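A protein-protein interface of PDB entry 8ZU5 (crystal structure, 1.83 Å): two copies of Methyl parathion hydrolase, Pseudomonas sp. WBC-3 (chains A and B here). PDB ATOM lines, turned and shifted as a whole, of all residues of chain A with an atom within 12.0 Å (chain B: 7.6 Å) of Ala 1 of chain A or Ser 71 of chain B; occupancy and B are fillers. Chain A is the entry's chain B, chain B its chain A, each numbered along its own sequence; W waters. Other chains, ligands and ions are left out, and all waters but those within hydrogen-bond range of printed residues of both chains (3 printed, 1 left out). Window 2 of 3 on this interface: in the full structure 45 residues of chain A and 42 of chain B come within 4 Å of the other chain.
ND2 of Asn 68 of chain B is in hydrogen-bond range of O of Ala 2 of chain A (3.2 Å). O of Pro 3 of chain A is in hydrogen-bond range of ND2 of Asn 68 of chain B, at 3.2 Å. The backbone carbonyl oxygen (O) of Asn 68 of chain B is in hydrogen-bond range of the side-chain amide nitrogen (NE2) of Gln 4 of chain A, 3.0 Å away. O of Ser 71 of chain B lies within hydrogen-bond range of N of Ala 1 of chain A, 3.4 Å away.
The backbone NH (N) of Gly 70 of chain B is in hydrogen-bond range of the side-chain amide oxygen (OD1) of Asn 68 of chain B (2.9 Å). The backbone NH of Ser 71 of chain B lies close to the side-chain hydroxyl of Thr 69 of chain B. The guanidinium group (NE) of Arg 6 of chain A sits at hydrogen-bond distance from the side-chain amide oxygen (OE1) of Gln 4 of chain A (2.8 Å).
Among the printed residues, merely in contact across the chains: Ala 2 of chain A with Gln 104 of chain B (3.6 Å), Gln 4 of chain A with Gly 70 of chain B (3.7 Å) and Gln 4 of chain A with Phe 20 of chain B (3.9 Å).
Of chain B, only Ser 71 (3.4 Å) comes within 4 Å of Ala 1 of chain A. Of the printed residues of chain B, Ala 2 of chain A touches Asn 68 and Gln 104. Of the printed residues of chain B, Pro 3 of chain A touches Asn 68 (3.2 Å). Printed residues of chain B within 4 Å of Gln 4 of chain A: Phe 20, Asn 68 and Gly 70. Of the printed residues of chain A, Phe 20 of chain B touches Gln 4. Val 67 of chain B touches none of the printed residues of chain A. Asn 68 of chain B touches three residues of chain A. Thr 69 of chain B touches none of the printed residues of chain A. Of chain A, only Gln 4 comes within 4 Å of Gly 70 of chain B. Of chain A, only Ala 1 comes within 4 Å of Ser 71 of chain B. Lys 72 of chain B touches none of the printed residues of chain A. No residue of chain A comes within 4 Å of Leu 73 of chain B. Printed residues of chain A within 4 Å of Gln 104 of chain B: Ala 2 (3.6 Å). The nearest residue of chain B that does not touch Ala 1 of chain A is Gly 70 of chain B (4.3 Å). The nearest residue of chain A that does not touch Ser 71 of chain B is Ala 2 of chain A (5.6 Å).
Of the 6 printed residues of chain A, 4 touch a printed residue of chain B. Hydrophobic or aromatic side chains of chain A that line the printed part of chain B: Ala 2. Printed residues of chain B that touch a printed residue of chain A: Phe 20, Asn 68, Gly 70, Ser 71 and Gln 104. Among the printed residues, 7 pairs touch across the chains.
No position is printed for both chains. Of the 7 pairs that touch across the chains among the printed residues, none has its exchanged pair printed and touching as well.
Water W2 lies within hydrogen-bond range of N of Ala 2 of chain A (2.7 Å), N of Ala 1 of chain A (2.8 Å) and OD2 of Asp 106 of chain B (3.1 Å). Water W3 lies within hydrogen-bond range of O of Ala 2 of chain A (2.8 Å) and O of Gly 70 of chain B (2.9 Å). Water W1 bridges the guanidinium group (NH2) of Arg 6 of chain A and the backbone carbonyl oxygen (O) of Phe 20 of chain B.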
ATOM      1  N   ALA A   1      23.197 -29.741   6.046  1.00  0.00           N
ATOM      2  CA  ALA A   1      24.536 -30.257   5.824  1.00  0.00           C
ATOM      3  C   ALA A   1      25.583 -29.209   6.194  1.00  0.00           C
ATOM      4  O   ALA A   1      26.744 -29.556   6.401  1.00  0.00           O
ATOM      5  CB  ALA A   1      24.720 -30.736   4.347  1.00  0.00           C
ATOM      6  N   ALA A   2      25.186 -27.938   6.295  1.00  0.00           N
ATOM      7  CA  ALA A   2      26.077 -26.946   6.895  1.00  0.00           C
ATOM      8  C   ALA A   2      26.312 -27.321   8.352  1.00  0.00           C
ATOM      9  O   ALA A   2      25.343 -27.468   9.108  1.00  0.00           O
ATOM     10  CB  ALA A   2      25.483 -25.541   6.807  1.00  0.00           C
ATOM     11  N   PRO A   3      27.561 -27.481   8.783  1.00  0.00           N
ATOM     12  CA  PRO A   3      27.817 -27.814  10.186  1.00  0.00           C
ATOM     13  C   PRO A   3      27.366 -26.703  11.132  1.00  0.00           C
ATOM     14  O   PRO A   3      27.412 -25.513  10.810  1.00  0.00           O
ATOM     15  CB  PRO A   3      29.339 -28.001  10.227  1.00  0.00           C
ATOM     16  CG  PRO A   3      29.842 -27.135   9.100  1.00  0.00           C
ATOM     17  CD  PRO A   3      28.808 -27.289   8.021  1.00  0.00           C
ATOM     18  N   GLN A   4      26.914 -27.106  12.313  1.00  0.00           N
ATOM     19  CA  GLN A   4      26.749 -26.133  13.385  1.00  0.00           C
ATOM     20  C   GLN A   4      28.121 -25.692  13.885  1.00  0.00           C
ATOM     21  O   GLN A   4      29.053 -26.493  13.967  1.00  0.00           O
ATOM     22  CB  GLN A   4      25.920 -26.723  14.531  1.00  0.00           C
ATOM     23  CG  GLN A   4      24.488 -27.073  14.130  1.00  0.00           C
ATOM     24  CD  GLN A   4      23.629 -27.580  15.280  1.00  0.00           C
ATOM     25  OE1 GLN A   4      24.146 -28.022  16.311  1.00  0.00           O
ATOM     26  NE2 GLN A   4      22.309 -27.473  15.128  1.00  0.00           N
ATOM     27  N   VAL A   5      28.255 -24.398  14.179  1.00  0.00           N
ATOM     28  CA  VAL A   5      29.526 -23.847  14.636  1.00  0.00           C
ATOM     29  C   VAL A   5      29.665 -24.009  16.137  1.00  0.00           C
ATOM     30  O   VAL A   5      30.706 -24.466  16.631  1.00  0.00           O
ATOM     31  CB  VAL A   5      29.637 -22.371  14.212  1.00  0.00           C
ATOM     32  CG1 VAL A   5      30.977 -21.794  14.629  1.00  0.00           C
ATOM     33  CG2 VAL A   5      29.438 -22.256  12.711  1.00  0.00           C
ATOM     34  N   ARG A   6      28.599 -23.638  16.871  1.00  0.00           N
ATOM     35  CA  ARG A   6      28.487 -23.840  18.317  1.00  0.00           C
ATOM     36  C   ARG A   6      29.642 -23.235  19.105  1.00  0.00           C
ATOM     37  O   ARG A   6      30.144 -23.830  20.050  1.00  0.00           O
ATOM     38  CB  ARG A   6      28.334 -25.314  18.674  1.00  0.00           C
ATOM     39  CG  ARG A   6      26.936 -25.837  18.433  1.00  0.00           C
ATOM     40  CD  ARG A   6      26.751 -27.135  19.152  1.00  0.00           C
ATOM     41  NE  ARG A   6      25.490 -27.766  18.799  1.00  0.00           N
ATOM     42  CZ  ARG A   6      24.692 -28.364  19.671  1.00  0.00           C
ATOM     43  NH1 ARG A   6      24.995 -28.406  20.963  1.00  0.00           N
ATOM     44  NH2 ARG A   6      23.570 -28.946  19.234  1.00  0.00           N
ATOM     45  N   PHE B  20      18.738 -27.359  17.989  1.00  0.00           N
ATOM     46  CA  PHE B  20      19.012 -26.340  16.987  1.00  0.00           C
ATOM     47  C   PHE B  20      20.021 -25.318  17.499  1.00  0.00           C
ATOM     48  O   PHE B  20      20.129 -25.046  18.700  1.00  0.00           O
ATOM     49  CB  PHE B  20      17.761 -25.565  16.565  1.00  0.00           C
ATOM     50  CG  PHE B  20      16.681 -26.392  15.917  1.00  0.00           C
ATOM     51  CD1 PHE B  20      16.895 -27.700  15.564  1.00  0.00           C
ATOM     52  CD2 PHE B  20      15.453 -25.808  15.612  1.00  0.00           C
ATOM     53  CE1 PHE B  20      15.885 -28.427  14.966  1.00  0.00           C
ATOM     54  CE2 PHE B  20      14.458 -26.524  15.001  1.00  0.00           C
ATOM     55  CZ  PHE B  20      14.672 -27.826  14.677  1.00  0.00           C
ATOM     56  N   VAL B  67      18.939 -19.982  11.883  1.00  0.00           N
ATOM     57  CA  VAL B  67      18.525 -21.225  12.509  1.00  0.00           C
ATOM     58  C   VAL B  67      19.237 -22.334  11.762  1.00  0.00           C
ATOM     59  O   VAL B  67      18.992 -22.540  10.565  1.00  0.00           O
ATOM     60  CB  VAL B  67      16.998 -21.435  12.469  1.00  0.00           C
ATOM     61  CG1 VAL B  67      16.621 -22.730  13.176  1.00  0.00           C
ATOM     62  CG2 VAL B  67      16.223 -20.224  13.071  1.00  0.00           C
ATOM     63  N   ASN B  68      20.117 -23.040  12.452  1.00  0.00           N
ATOM     64  CA  ASN B  68      20.757 -24.225  11.895  1.00  0.00           C
ATOM     65  C   ASN B  68      20.097 -25.399  12.601  1.00  0.00           C
ATOM     66  O   ASN B  68      20.378 -25.669  13.775  1.00  0.00           O
ATOM     67  CB  ASN B  68      22.277 -24.194  12.095  1.00  0.00           C
ATOM     68  CG  ASN B  68      22.979 -25.304  11.340  1.00  0.00           C
ATOM     69  OD1 ASN B  68      22.402 -26.349  11.122  1.00  0.00           O
ATOM     70  ND2 ASN B  68      24.237 -25.090  10.975  1.00  0.00           N
ATOM     71  N   THR B  69      19.189 -26.079  11.894  1.00  0.00           N
ATOM     72  CA  THR B  69      18.486 -27.212  12.485  1.00  0.00           C
ATOM     73  C   THR B  69      19.345 -28.464  12.538  1.00  0.00           C
ATOM     74  O   THR B  69      18.903 -29.467  13.097  1.00  0.00           O
ATOM     75  CB  THR B  69      17.193 -27.524  11.713  1.00  0.00           C
ATOM     76  OG1 THR B  69      17.536 -28.104  10.445  1.00  0.00           O
ATOM     77  CG2 THR B  69      16.369 -26.250  11.491  1.00  0.00           C
ATOM     78  N   GLY B  70      20.570 -28.404  12.003  1.00  0.00           N
ATOM     79  CA  GLY B  70      21.428 -29.549  11.847  1.00  0.00           C
ATOM     80  C   GLY B  70      21.331 -30.179  10.483  1.00  0.00           C
ATOM     81  O   GLY B  70      22.265 -30.857  10.059  1.00  0.00           O
ATOM     82  N   SER B  71      20.247 -29.891   9.770  1.00  0.00           N
ATOM     83  CA  SER B  71      19.952 -30.418   8.449  1.00  0.00           C
ATOM     84  C   SER B  71      19.695 -29.315   7.442  1.00  0.00           C
ATOM     85  O   SER B  71      19.851 -29.552   6.238  1.00  0.00           O
ATOM     86  CB  SER B  71      18.706 -31.315   8.507  1.00  0.00           C
ATOM     87  OG  SER B  71      19.019 -32.603   8.990  1.00  0.00           O
ATOM     88  N   LYS B  72      19.283 -28.133   7.889  1.00  0.00           N
ATOM     89  CA  LYS B  72      19.025 -26.985   7.037  1.00  0.00           C
ATOM     90  C   LYS B  72      19.555 -25.741   7.724  1.00  0.00           C
ATOM     91  O   LYS B  72      19.607 -25.669   8.953  1.00  0.00           O
ATOM     92  CB  LYS B  72      17.529 -26.793   6.729  1.00  0.00           C
ATOM     93  CG  LYS B  72      16.915 -27.902   5.884  1.00  0.00           C
ATOM     94  CD  LYS B  72      17.451 -27.826   4.423  1.00  0.00           C
ATOM     95  CE  LYS B  72      16.891 -28.924   3.502  1.00  0.00           C
ATOM     96  NZ  LYS B  72      15.449 -28.733   3.203  1.00  0.00           N
ATOM     97  N   LEU B  73      19.949 -24.770   6.912  1.00  0.00           N
ATOM     98  CA  LEU B  73      20.394 -23.464   7.369  1.00  0.00           C
ATOM     99  C   LEU B  73      19.379 -22.447   6.859  1.00  0.00           C
ATOM    100  O   LEU B  73      19.260 -22.242   5.646  1.00  0.00           O
ATOM    101  CB  LEU B  73      21.819 -23.177   6.874  1.00  0.00           C
ATOM    102  CG  LEU B  73      22.409 -21.946   7.563  1.00  0.00           C
ATOM    103  CD1 LEU B  73      22.590 -22.170   9.075  1.00  0.00           C
ATOM    104  CD2 LEU B  73      23.737 -21.538   6.902  1.00  0.00           C
ATOM    105  N   VAL B  74      18.626 -21.850   7.786  1.00  0.00           N
ATOM    106  CA  VAL B  74      17.508 -20.941   7.509  1.00  0.00           C
ATOM    107  C   VAL B  74      17.784 -19.583   8.132  1.00  0.00           C
ATOM    108  O   VAL B  74      18.162 -19.502   9.300  1.00  0.00           O
ATOM    109  CB  VAL B  74      16.159 -21.483   8.037  1.00  0.00           C
ATOM    110  CG1 VAL B  74      15.043 -20.480   7.721  1.00  0.00           C
ATOM    111  CG2 VAL B  74      15.795 -22.809   7.391  1.00  0.00           C
ATOM    112  N   GLN B 104      25.708 -21.008   2.027  1.00  0.00           N
ATOM    113  CA  GLN B 104      25.232 -22.139   2.806  1.00  0.00           C
ATOM    114  C   GLN B 104      23.761 -22.033   3.162  1.00  0.00           C
ATOM    115  O   GLN B 104      23.161 -23.048   3.528  1.00  0.00           O
ATOM    116  CB  GLN B 104      26.067 -22.300   4.077  1.00  0.00           C
ATOM    117  CG  GLN B 104      27.519 -22.752   3.839  1.00  0.00           C
ATOM    118  CD  GLN B 104      28.298 -22.875   5.151  1.00  0.00           C
ATOM    119  OE1 GLN B 104      28.628 -21.871   5.790  1.00  0.00           O
ATOM    120  NE2 GLN B 104      28.582 -24.114   5.564  1.00  0.00           N
ATOM    121  N   ASP B 106      20.035 -22.261   3.028  1.00  0.00           N
ATOM    122  CA  ASP B 106      19.106 -23.062   2.221  1.00  0.00           C
ATOM    123  C   ASP B 106      17.788 -22.334   1.944  1.00  0.00           C
ATOM    124  O   ASP B 106      17.216 -22.469   0.851  1.00  0.00           O
ATOM    125  CB  ASP B 106      18.800 -24.372   2.952  1.00  0.00           C
ATOM    126  CG  ASP B 106      20.014 -25.264   3.098  1.00  0.00           C
ATOM    127  OD1 ASP B 106      20.668 -25.538   2.076  1.00  0.00           O
ATOM    128  OD2 ASP B 106      20.355 -25.644   4.251  1.00  0.00           O
ATOM    129  N   VAL B 188      10.084 -25.961   6.780  1.00  0.00           N
ATOM    130  CA  VAL B 188      11.133 -26.867   7.245  1.00  0.00           C
ATOM    131  C   VAL B 188      10.745 -27.488   8.588  1.00  0.00           C
ATOM    132  O   VAL B 188      10.226 -26.774   9.462  1.00  0.00           O
ATOM    133  CB  VAL B 188      12.460 -26.093   7.340  1.00  0.00           C
ATOM    134  CG1 VAL B 188      13.379 -26.665   8.395  1.00  0.00           C
ATOM    135  CG2 VAL B 188      13.151 -26.067   5.971  1.00  0.00           C
ATOM    136  N   PRO B 189      10.920 -28.834   8.779  1.00  0.00           N
ATOM    137  CA  PRO B 189      10.721 -29.434  10.108  1.00  0.00           C
ATOM    138  C   PRO B 189      11.361 -28.616  11.213  1.00  0.00           C
ATOM    139  O   PRO B 189      12.562 -28.361  11.177  1.00  0.00           O
ATOM    140  CB  PRO B 189      11.402 -30.802   9.975  1.00  0.00           C
ATOM    141  CG  PRO B 189      11.181 -31.160   8.542  1.00  0.00           C
ATOM    142  CD  PRO B 189      11.346 -29.843   7.790  1.00  0.00           C
HETATM  143  O   HOH W   1      21.359 -27.302  20.258  1.00  0.00           O
HETATM  144  O   HOH W   2      22.781 -26.986   5.649  1.00  0.00           O
HETATM  145  O   HOH W   3      24.984 -29.972  10.411  1.00  0.00           O
